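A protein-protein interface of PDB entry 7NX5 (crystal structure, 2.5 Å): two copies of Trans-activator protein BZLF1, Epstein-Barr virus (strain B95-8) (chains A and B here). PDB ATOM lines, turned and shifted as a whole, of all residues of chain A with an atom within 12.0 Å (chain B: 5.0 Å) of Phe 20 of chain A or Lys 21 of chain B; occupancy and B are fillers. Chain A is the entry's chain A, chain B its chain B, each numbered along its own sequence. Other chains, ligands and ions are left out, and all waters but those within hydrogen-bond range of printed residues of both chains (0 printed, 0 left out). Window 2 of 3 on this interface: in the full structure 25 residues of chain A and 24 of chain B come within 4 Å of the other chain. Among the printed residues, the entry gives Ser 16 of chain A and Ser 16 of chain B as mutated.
Among the printed residues, merely in contact across the chains: Phe 20 of chain A with Phe 20 of chain B, Phe 20 of chain A with Lys 21 of chain B, Lys 21 of chain A with Phe 20 of chain B, Leu 23 of chain A with Leu 24 of chain B, Leu 24 of chain A with Phe 20 of chain B, Leu 24 of chain A with Leu 23 of chain B, Leu 24 of chain A with Leu 24 of chain B and Tyr 27 of chain A with Leu 24 of chain B.
Phe 20 of chain A touches just these residues of chain B: Phe 20 and Lys 21.
Printed residues of chain A within 4 Å of Lys 21 of chain B: Phe 20 (3.6 Å).
Ala 18 of chain B touches none of the printed residues of chain A.
Phe 20 of chain B touches just these residues of chain A: Phe 20, Lys 21 and Leu 24.
No residue of chain A comes within 4 Å of Gln 22 of chain B.
Printed residues of chain A within 4 Å of Leu 23 of chain B: Leu 24.
Of the printed residues of chain B, Leu 23 of chain A touches Leu 24 (3.99 Å).
Printed residues of chain A within 4 Å of Leu 24 of chain B: Leu 23 (3.99 Å), Leu 24 (3.8 Å) and Tyr 27 (3.6 Å).
The nearest residue of chain B that does not touch Phe 20 of chain A is Leu 24 of chain B (4.3 Å).
The nearest printed residue of chain B that does not touch Leu 24 of chain A is Gln 25 of chain B (5.9 Å).
Hydrophobic or aromatic side chains of chain B within 4 Å of the printed part of chain A: Phe 20 and Leu 24.
Of the 19 printed residues of chain A, 5 touch a printed residue of chain B.
Printed residues of chain A that touch a printed residue of chain B: Phe 20, Lys 21, Leu 23, Leu 24 and Tyr 27.
Among the printed residues, no Asp or Glu carboxylate lies within 4 Å of a Lys or Arg side-chain nitrogen of the other chain.
Phe 20 of chain A touches its own counterpart, Phe 20 of chain B.
Phe 20 of chain A touches Lys 21 of chain B, and with the chains exchanged Lys 21 of chain A touches Phe 20 of chain B.
Leu 24 of chain A touches Phe 20 of chain B, but with the chains exchanged Phe 20 of chain A does not touch Leu 24 of chain B (4.3 Å).
Leu 24 of chain A touches its own counterpart, Leu 24 of chain B.
Positions printed for both chains: 16, 17, 18, 19, 20, 21, 22, 23, 24 and 25.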
ATOM      1  N   VAL A  11      28.124 -36.279 -11.362  1.00  0.00           N
ATOM      2  CA  VAL A  11      26.787 -36.730 -11.744  1.00  0.00           C
ATOM      3  C   VAL A  11      25.701 -35.858 -11.125  1.00  0.00           C
ATOM      4  O   VAL A  11      24.719 -35.488 -11.785  1.00  0.00           O
ATOM      5  CB  VAL A  11      26.613 -38.205 -11.341  1.00  0.00           C
ATOM      6  CG1 VAL A  11      25.154 -38.611 -11.379  1.00  0.00           C
ATOM      7  CG2 VAL A  11      27.496 -39.091 -12.228  1.00  0.00           C
ATOM      8  N   ALA A  12      25.856 -35.499  -9.841  1.00  0.00           N
ATOM      9  CA  ALA A  12      24.800 -34.751  -9.169  1.00  0.00           C
ATOM     10  C   ALA A  12      24.695 -33.337  -9.712  1.00  0.00           C
ATOM     11  O   ALA A  12      23.587 -32.827  -9.938  1.00  0.00           O
ATOM     12  CB  ALA A  12      25.028 -34.721  -7.659  1.00  0.00           C
ATOM     13  N   SER A  13      25.837 -32.682  -9.916  1.00  0.00           N
ATOM     14  CA  SER A  13      25.791 -31.334 -10.466  1.00  0.00           C
ATOM     15  C   SER A  13      25.194 -31.334 -11.868  1.00  0.00           C
ATOM     16  O   SER A  13      24.371 -30.464 -12.202  1.00  0.00           O
ATOM     17  CB  SER A  13      27.177 -30.695 -10.437  1.00  0.00           C
ATOM     18  OG  SER A  13      27.324 -30.005  -9.196  1.00  0.00           O
ATOM     19  N   ARG A  14      25.573 -32.314 -12.697  1.00  0.00           N
ATOM     20  CA  ARG A  14      24.992 -32.387 -14.029  1.00  0.00           C
ATOM     21  C   ARG A  14      23.482 -32.626 -13.950  1.00  0.00           C
ATOM     22  O   ARG A  14      22.693 -32.013 -14.688  1.00  0.00           O
ATOM     23  CB  ARG A  14      25.715 -33.459 -14.848  1.00  0.00           C
ATOM     24  CG  ARG A  14      27.221 -33.172 -15.029  1.00  0.00           C
ATOM     25  CD  ARG A  14      27.696 -33.197 -16.483  1.00  0.00           C
ATOM     26  NE  ARG A  14      28.217 -34.511 -16.880  1.00  0.00           N
ATOM     27  CZ  ARG A  14      28.864 -34.781 -18.018  1.00  0.00           C
ATOM     28  NH1 ARG A  14      29.102 -33.834 -18.919  1.00  0.00           N
ATOM     29  NH2 ARG A  14      29.283 -36.022 -18.256  1.00  0.00           N
ATOM     30  N   LYS A  15      23.053 -33.430 -12.978  1.00  0.00           N
ATOM     31  CA  LYS A  15      21.627 -33.661 -12.798  1.00  0.00           C
ATOM     32  C   LYS A  15      20.888 -32.368 -12.482  1.00  0.00           C
ATOM     33  O   LYS A  15      19.901 -32.032 -13.139  1.00  0.00           O
ATOM     34  CB  LYS A  15      21.398 -34.697 -11.691  1.00  0.00           C
ATOM     35  CG  LYS A  15      19.927 -34.980 -11.431  1.00  0.00           C
ATOM     36  CD  LYS A  15      19.707 -36.284 -10.651  1.00  0.00           C
ATOM     37  CE  LYS A  15      18.213 -36.486 -10.359  1.00  0.00           C
ATOM     38  NZ  LYS A  15      17.908 -37.639  -9.455  1.00  0.00           N
ATOM     39  N   SER A  16      21.350 -31.633 -11.473  1.00  0.00           N
ATOM     40  CA  SER A  16      20.565 -30.516 -10.949  1.00  0.00           C
ATOM     41  C   SER A  16      20.586 -29.319 -11.895  1.00  0.00           C
ATOM     42  O   SER A  16      19.588 -28.581 -12.016  1.00  0.00           O
ATOM     43  CB  SER A  16      21.088 -30.113  -9.571  1.00  0.00           C
ATOM     44  OG  SER A  16      21.274 -28.719  -9.494  1.00  0.00           O
ATOM     45  N   ARG A  17      21.710 -29.112 -12.578  1.00  0.00           N
ATOM     46  CA  ARG A  17      21.746 -28.032 -13.549  1.00  0.00           C
ATOM     47  C   ARG A  17      20.831 -28.344 -14.721  1.00  0.00           C
ATOM     48  O   ARG A  17      20.068 -27.470 -15.167  1.00  0.00           O
ATOM     49  CB  ARG A  17      23.193 -27.774 -13.978  1.00  0.00           C
ATOM     50  CG  ARG A  17      24.045 -27.231 -12.797  1.00  0.00           C
ATOM     51  CD  ARG A  17      25.565 -27.169 -13.096  1.00  0.00           C
ATOM     52  NE  ARG A  17      26.266 -26.373 -12.096  1.00  0.00           N
ATOM     53  CZ  ARG A  17      27.561 -26.464 -11.787  1.00  0.00           C
ATOM     54  NH1 ARG A  17      28.351 -27.352 -12.392  1.00  0.00           N
ATOM     55  NH2 ARG A  17      28.063 -25.668 -10.834  1.00  0.00           N
ATOM     56  N   ALA A  18      20.850 -29.602 -15.196  1.00  0.00           N
ATOM     57  CA  ALA A  18      19.890 -30.026 -16.201  1.00  0.00           C
ATOM     58  C   ALA A  18      18.453 -29.864 -15.701  1.00  0.00           C
ATOM     59  O   ALA A  18      17.557 -29.499 -16.472  1.00  0.00           O
ATOM     60  CB  ALA A  18      20.178 -31.480 -16.601  1.00  0.00           C
ATOM     61  N   LYS A  19      18.221 -30.124 -14.414  1.00  0.00           N
ATOM     62  CA  LYS A  19      16.880 -29.991 -13.845  1.00  0.00           C
ATOM     63  C   LYS A  19      16.342 -28.576 -14.009  1.00  0.00           C
ATOM     64  O   LYS A  19      15.235 -28.368 -14.531  1.00  0.00           O
ATOM     65  CB  LYS A  19      16.903 -30.369 -12.361  1.00  0.00           C
ATOM     66  CG  LYS A  19      15.643 -29.968 -11.589  1.00  0.00           C
ATOM     67  CD  LYS A  19      15.669 -30.485 -10.154  1.00  0.00           C
ATOM     68  CE  LYS A  19      14.335 -30.266  -9.488  1.00  0.00           C
ATOM     69  NZ  LYS A  19      14.209 -31.077  -8.225  1.00  0.00           N
ATOM     70  N   PHE A  20      17.108 -27.584 -13.552  1.00  0.00           N
ATOM     71  CA  PHE A  20      16.652 -26.199 -13.676  1.00  0.00           C
ATOM     72  C   PHE A  20      16.461 -25.797 -15.141  1.00  0.00           C
ATOM     73  O   PHE A  20      15.465 -25.155 -15.491  1.00  0.00           O
ATOM     74  CB  PHE A  20      17.626 -25.240 -12.986  1.00  0.00           C
ATOM     75  CG  PHE A  20      17.384 -25.087 -11.494  1.00  0.00           C
ATOM     76  CD1 PHE A  20      16.434 -25.864 -10.845  1.00  0.00           C
ATOM     77  CD2 PHE A  20      18.095 -24.151 -10.745  1.00  0.00           C
ATOM     78  CE1 PHE A  20      16.207 -25.716  -9.478  1.00  0.00           C
ATOM     79  CE2 PHE A  20      17.870 -23.998  -9.383  1.00  0.00           C
ATOM     80  CZ  PHE A  20      16.930 -24.784  -8.750  1.00  0.00           C
ATOM     81  N   LYS A  21      17.416 -26.158 -16.005  1.00  0.00           N
ATOM     82  CA  LYS A  21      17.325 -25.759 -17.408  1.00  0.00           C
ATOM     83  C   LYS A  21      16.078 -26.330 -18.085  1.00  0.00           C
ATOM     84  O   LYS A  21      15.354 -25.612 -18.801  1.00  0.00           O
ATOM     85  CB  LYS A  21      18.597 -26.182 -18.142  1.00  0.00           C
ATOM     86  CG  LYS A  21      19.797 -25.220 -17.901  1.00  0.00           C
ATOM     87  CD  LYS A  21      20.458 -24.787 -19.216  1.00  0.00           C
ATOM     88  CE  LYS A  21      21.757 -23.971 -19.018  1.00  0.00           C
ATOM     89  NZ  LYS A  21      21.569 -22.542 -18.578  1.00  0.00           N
ATOM     90  N   GLN A  22      15.790 -27.618 -17.868  1.00  0.00           N
ATOM     91  CA  GLN A  22      14.600 -28.177 -18.504  1.00  0.00           C
ATOM     92  C   GLN A  22      13.332 -27.606 -17.886  1.00  0.00           C
ATOM     93  O   GLN A  22      12.303 -27.503 -18.560  1.00  0.00           O
ATOM     94  CB  GLN A  22      14.582 -29.694 -18.421  1.00  0.00           C
ATOM     95  CG  GLN A  22      14.777 -30.379 -19.783  1.00  0.00           C
ATOM     96  CD  GLN A  22      15.089 -31.868 -19.664  1.00  0.00           C
ATOM     97  OE1 GLN A  22      14.508 -32.579 -18.843  1.00  0.00           O
ATOM     98  NE2 GLN A  22      16.009 -32.344 -20.485  1.00  0.00           N
ATOM     99  N   LEU A  23      13.377 -27.230 -16.606  1.00  0.00           N
ATOM    100  CA  LEU A  23      12.190 -26.639 -16.004  1.00  0.00           C
ATOM    101  C   LEU A  23      11.892 -25.279 -16.641  1.00  0.00           C
ATOM    102  O   LEU A  23      10.727 -24.953 -16.935  1.00  0.00           O
ATOM    103  CB  LEU A  23      12.389 -26.516 -14.493  1.00  0.00           C
ATOM    104  CG  LEU A  23      11.257 -26.413 -13.492  1.00  0.00           C
ATOM    105  CD1 LEU A  23      10.701 -27.787 -13.268  1.00  0.00           C
ATOM    106  CD2 LEU A  23      11.791 -25.824 -12.213  1.00  0.00           C
ATOM    107  N   LEU A  24      12.941 -24.481 -16.865  1.00  0.00           N
ATOM    108  CA  LEU A  24      12.783 -23.224 -17.590  1.00  0.00           C
ATOM    109  C   LEU A  24      12.154 -23.456 -18.962  1.00  0.00           C
ATOM    110  O   LEU A  24      11.157 -22.808 -19.323  1.00  0.00           O
ATOM    111  CB  LEU A  24      14.131 -22.547 -17.736  1.00  0.00           C
ATOM    112  CG  LEU A  24      14.097 -21.185 -18.426  1.00  0.00           C
ATOM    113  CD1 LEU A  24      12.970 -20.342 -17.869  1.00  0.00           C
ATOM    114  CD2 LEU A  24      15.450 -20.484 -18.230  1.00  0.00           C
ATOM    115  N   GLN A  25      12.732 -24.369 -19.753  1.00  0.00           N
ATOM    116  CA  GLN A  25      12.135 -24.687 -21.050  1.00  0.00           C
ATOM    117  C   GLN A  25      10.671 -25.086 -20.909  1.00  0.00           C
ATOM    118  O   GLN A  25       9.814 -24.673 -21.704  1.00  0.00           O
ATOM    119  CB  GLN A  25      12.909 -25.810 -21.743  1.00  0.00           C
ATOM    120  CG  GLN A  25      14.139 -25.328 -22.467  1.00  0.00           C
ATOM    121  CD  GLN A  25      13.897 -24.053 -23.256  1.00  0.00           C
ATOM    122  OE1 GLN A  25      14.627 -23.074 -23.112  1.00  0.00           O
ATOM    123  NE2 GLN A  25      12.889 -24.068 -24.116  1.00  0.00           N
ATOM    124  N   HIS A  26      10.379 -25.928 -19.920  1.00  0.00           N
ATOM    125  CA  HIS A  26       9.029 -26.400 -19.672  1.00  0.00           C
ATOM    126  C   HIS A  26       8.050 -25.235 -19.505  1.00  0.00           C
ATOM    127  O   HIS A  26       6.983 -25.210 -20.124  1.00  0.00           O
ATOM    128  CB  HIS A  26       9.041 -27.262 -18.419  1.00  0.00           C
ATOM    129  CG  HIS A  26       7.684 -27.605 -17.908  1.00  0.00           C
ATOM    130  ND1 HIS A  26       7.298 -27.356 -16.612  1.00  0.00           N
ATOM    131  CD2 HIS A  26       6.619 -28.176 -18.516  1.00  0.00           C
ATOM    132  CE1 HIS A  26       6.056 -27.771 -16.434  1.00  0.00           C
ATOM    133  NE2 HIS A  26       5.624 -28.275 -17.576  1.00  0.00           N
ATOM    134  N   TYR A  27       8.396 -24.296 -18.624  1.00  0.00           N
ATOM    135  CA  TYR A  27       7.561 -23.109 -18.433  1.00  0.00           C
ATOM    136  C   TYR A  27       7.348 -22.384 -19.746  1.00  0.00           C
ATOM    137  O   TYR A  27       6.235 -21.942 -20.047  1.00  0.00           O
ATOM    138  CB  TYR A  27       8.198 -22.146 -17.428  1.00  0.00           C
ATOM    139  CG  TYR A  27       8.236 -22.658 -16.025  1.00  0.00           C
ATOM    140  CD1 TYR A  27       7.397 -23.682 -15.617  1.00  0.00           C
ATOM    141  CD2 TYR A  27       9.130 -22.127 -15.100  1.00  0.00           C
ATOM    142  CE1 TYR A  27       7.447 -24.161 -14.308  1.00  0.00           C
ATOM    143  CE2 TYR A  27       9.173 -22.589 -13.799  1.00  0.00           C
ATOM    144  CZ  TYR A  27       8.342 -23.602 -13.412  1.00  0.00           C
ATOM    145  OH  TYR A  27       8.390 -24.045 -12.114  1.00  0.00           O
ATOM    146  N   ARG A  28       8.430 -22.189 -20.505  1.00  0.00           N
ATOM    147  CA  ARG A  28       8.319 -21.506 -21.786  1.00  0.00           C
ATOM    148  C   ARG A  28       7.319 -22.217 -22.693  1.00  0.00           C
ATOM    149  O   ARG A  28       6.526 -21.569 -23.391  1.00  0.00           O
ATOM    150  CB  ARG A  28       9.698 -21.385 -22.433  1.00  0.00           C
ATOM    151  CG  ARG A  28      10.354 -19.981 -22.248  1.00  0.00           C
ATOM    152  CD  ARG A  28      11.890 -20.052 -22.226  1.00  0.00           C
ATOM    153  NE  ARG A  28      12.552 -18.789 -22.565  1.00  0.00           N
ATOM    154  CZ  ARG A  28      13.841 -18.689 -22.901  1.00  0.00           C
ATOM    155  NH1 ARG A  28      14.614 -19.769 -22.941  1.00  0.00           N
ATOM    156  NH2 ARG A  28      14.368 -17.512 -23.212  1.00  0.00           N
ATOM    157  N   GLU A  29       7.270 -23.549 -22.616  1.00  0.00           N
ATOM    158  CA  GLU A  29       6.295 -24.271 -23.419  1.00  0.00           C
ATOM    159  C   GLU A  29       4.876 -24.093 -22.872  1.00  0.00           C
ATOM    160  O   GLU A  29       3.919 -23.946 -23.645  1.00  0.00           O
ATOM    161  CB  GLU A  29       6.671 -25.741 -23.508  1.00  0.00           C
ATOM    162  CG  GLU A  29       5.945 -26.433 -24.652  1.00  0.00           C
ATOM    163  CD  GLU A  29       5.794 -25.527 -25.885  1.00  0.00           C
ATOM    164  OE1 GLU A  29       6.816 -25.317 -26.594  1.00  0.00           O
ATOM    165  OE2 GLU A  29       4.658 -25.022 -26.136  1.00  0.00           O
ATOM    166  N   SER B  16      25.622 -14.580 -13.680  1.00  0.00           N
ATOM    167  CA  SER B  16      25.004 -15.600 -14.529  1.00  0.00           C
ATOM    168  C   SER B  16      23.982 -16.421 -13.749  1.00  0.00           C
ATOM    169  O   SER B  16      22.813 -16.559 -14.167  1.00  0.00           O
ATOM    170  CB  SER B  16      26.085 -16.499 -15.131  1.00  0.00           C
ATOM    171  OG  SER B  16      25.920 -16.614 -16.529  1.00  0.00           O
ATOM    172  N   ARG B  17      24.409 -16.974 -12.602  1.00  0.00           N
ATOM    173  CA  ARG B  17      23.460 -17.676 -11.726  1.00  0.00           C
ATOM    174  C   ARG B  17      22.212 -16.823 -11.432  1.00  0.00           C
ATOM    175  O   ARG B  17      21.082 -17.326 -11.466  1.00  0.00           O
ATOM    176  CB  ARG B  17      24.149 -18.083 -10.416  1.00  0.00           C
ATOM    177  CG  ARG B  17      25.224 -19.172 -10.535  1.00  0.00           C
ATOM    178  CD  ARG B  17      25.766 -19.623  -9.162  1.00  0.00           C
ATOM    179  NE  ARG B  17      26.490 -18.559  -8.420  1.00  0.00           N
ATOM    180  CZ  ARG B  17      27.786 -18.325  -8.562  1.00  0.00           C
ATOM    181  NH1 ARG B  17      28.511 -19.046  -9.413  1.00  0.00           N
ATOM    182  NH2 ARG B  17      28.351 -17.382  -7.874  1.00  0.00           N
ATOM    183  N   ALA B  18      22.395 -15.518 -11.190  1.00  0.00           N
ATOM    184  CA  ALA B  18      21.247 -14.654 -10.881  1.00  0.00           C
ATOM    185  C   ALA B  18      20.326 -14.482 -12.086  1.00  0.00           C
ATOM    186  O   ALA B  18      19.136 -14.796 -12.001  1.00  0.00           O
ATOM    187  CB  ALA B  18      21.717 -13.292 -10.370  1.00  0.00           C
ATOM    188  N   LYS B  19      20.866 -13.982 -13.208  1.00  0.00           N
ATOM    189  CA  LYS B  19      20.102 -13.789 -14.442  1.00  0.00           C
ATOM    190  C   LYS B  19      19.213 -14.975 -14.758  1.00  0.00           C
ATOM    191  O   LYS B  19      18.028 -14.815 -15.084  1.00  0.00           O
ATOM    192  CB  LYS B  19      21.061 -13.552 -15.612  1.00  0.00           C
ATOM    193  CG  LYS B  19      20.496 -13.947 -17.006  1.00  0.00           C
ATOM    194  CD  LYS B  19      21.587 -13.895 -18.103  1.00  0.00           C
ATOM    195  CE  LYS B  19      21.016 -13.913 -19.518  1.00  0.00           C
ATOM    196  NZ  LYS B  19      22.113 -13.577 -20.479  1.00  0.00           N
ATOM    197  N   PHE B  20      19.780 -16.182 -14.662  1.00  0.00           N
ATOM    198  CA  PHE B  20      19.020 -17.383 -14.999  1.00  0.00           C
ATOM    199  C   PHE B  20      17.970 -17.698 -13.943  1.00  0.00           C
ATOM    200  O   PHE B  20      16.904 -18.232 -14.266  1.00  0.00           O
ATOM    201  CB  PHE B  20      19.971 -18.577 -15.170  1.00  0.00           C
ATOM    202  CG  PHE B  20      19.276 -19.912 -15.171  1.00  0.00           C
ATOM    203  CD1 PHE B  20      18.884 -20.498 -16.360  1.00  0.00           C
ATOM    204  CD2 PHE B  20      19.015 -20.585 -13.981  1.00  0.00           C
ATOM    205  CE1 PHE B  20      18.241 -21.736 -16.363  1.00  0.00           C
ATOM    206  CE2 PHE B  20      18.364 -21.811 -13.976  1.00  0.00           C
ATOM    207  CZ  PHE B  20      17.980 -22.390 -15.165  1.00  0.00           C
ATOM    208  N   LYS B  21      18.264 -17.439 -12.665  1.00  0.00           N
ATOM    209  CA  LYS B  21      17.210 -17.607 -11.673  1.00  0.00           C
ATOM    210  C   LYS B  21      16.082 -16.599 -11.902  1.00  0.00           C
ATOM    211  O   LYS B  21      14.898 -16.924 -11.772  1.00  0.00           O
ATOM    212  CB  LYS B  21      17.803 -17.493 -10.275  1.00  0.00           C
ATOM    213  CG  LYS B  21      18.502 -18.799  -9.885  1.00  0.00           C
ATOM    214  CD  LYS B  21      18.987 -18.813  -8.441  1.00  0.00           C
ATOM    215  CE  LYS B  21      18.962 -20.226  -7.911  1.00  0.00           C
ATOM    216  NZ  LYS B  21      17.583 -20.795  -7.845  1.00  0.00           N
ATOM    217  N   GLN B  22      16.437 -15.380 -12.287  1.00  0.00           N
ATOM    218  CA  GLN B  22      15.435 -14.390 -12.629  1.00  0.00           C
ATOM    219  C   GLN B  22      14.562 -14.883 -13.773  1.00  0.00           C
ATOM    220  O   GLN B  22      13.339 -14.732 -13.744  1.00  0.00           O
ATOM    221  CB  GLN B  22      16.120 -13.091 -12.994  1.00  0.00           C
ATOM    222  CG  GLN B  22      15.449 -11.869 -12.423  1.00  0.00           C
ATOM    223  CD  GLN B  22      16.353 -10.644 -12.439  1.00  0.00           C
ATOM    224  OE1 GLN B  22      17.546 -10.723 -12.096  1.00  0.00           O
ATOM    225  NE2 GLN B  22      15.783  -9.496 -12.837  1.00  0.00           N
ATOM    226  N   LEU B  23      15.183 -15.468 -14.799  1.00  0.00           N
ATOM    227  CA  LEU B  23      14.429 -15.972 -15.941  1.00  0.00           C
ATOM    228  C   LEU B  23      13.519 -17.124 -15.537  1.00  0.00           C
ATOM    229  O   LEU B  23      12.339 -17.188 -15.926  1.00  0.00           O
ATOM    230  CB  LEU B  23      15.389 -16.424 -17.030  1.00  0.00           C
ATOM    231  CG  LEU B  23      15.404 -15.354 -18.100  1.00  0.00           C
ATOM    232  CD1 LEU B  23      16.067 -14.117 -17.554  1.00  0.00           C
ATOM    233  CD2 LEU B  23      16.090 -15.870 -19.339  1.00  0.00           C
ATOM    234  N   LEU B  24      14.059 -18.066 -14.773  1.00  0.00           N
ATOM    235  CA  LEU B  24      13.214 -19.133 -14.264  1.00  0.00           C
ATOM    236  C   LEU B  24      12.016 -18.553 -13.512  1.00  0.00           C
ATOM    237  O   LEU B  24      10.890 -19.016 -13.689  1.00  0.00           O
ATOM    238  CB  LEU B  24      14.053 -20.095 -13.411  1.00  0.00           C
ATOM    239  CG  LEU B  24      13.337 -21.294 -12.773  1.00  0.00           C
ATOM    240  CD1 LEU B  24      12.744 -22.289 -13.799  1.00  0.00           C
ATOM    241  CD2 LEU B  24      14.276 -22.002 -11.819  1.00  0.00           C
ATOM    242  N   GLN B  25      12.206 -17.461 -12.772  1.00  0.00           N
ATOM    243  CA  GLN B  25      11.090 -16.897 -12.007  1.00  0.00           C
ATOM    244  C   GLN B  25      10.073 -16.216 -12.921  1.00  0.00           C
ATOM    245  O   GLN B  25       8.864 -16.446 -12.814  1.00  0.00           O
ATOM    246  CB  GLN B  25      11.612 -15.898 -10.970  1.00  0.00           C
ATOM    247  CG  GLN B  25      12.420 -16.504  -9.824  1.00  0.00           C
ATOM    248  CD  GLN B  25      11.571 -17.327  -8.865  1.00  0.00           C
ATOM    249  OE1 GLN B  25      10.369 -17.525  -9.076  1.00  0.00           O
ATOM    250  NE2 GLN B  25      12.199 -17.816  -7.801  1.00  0.00           N
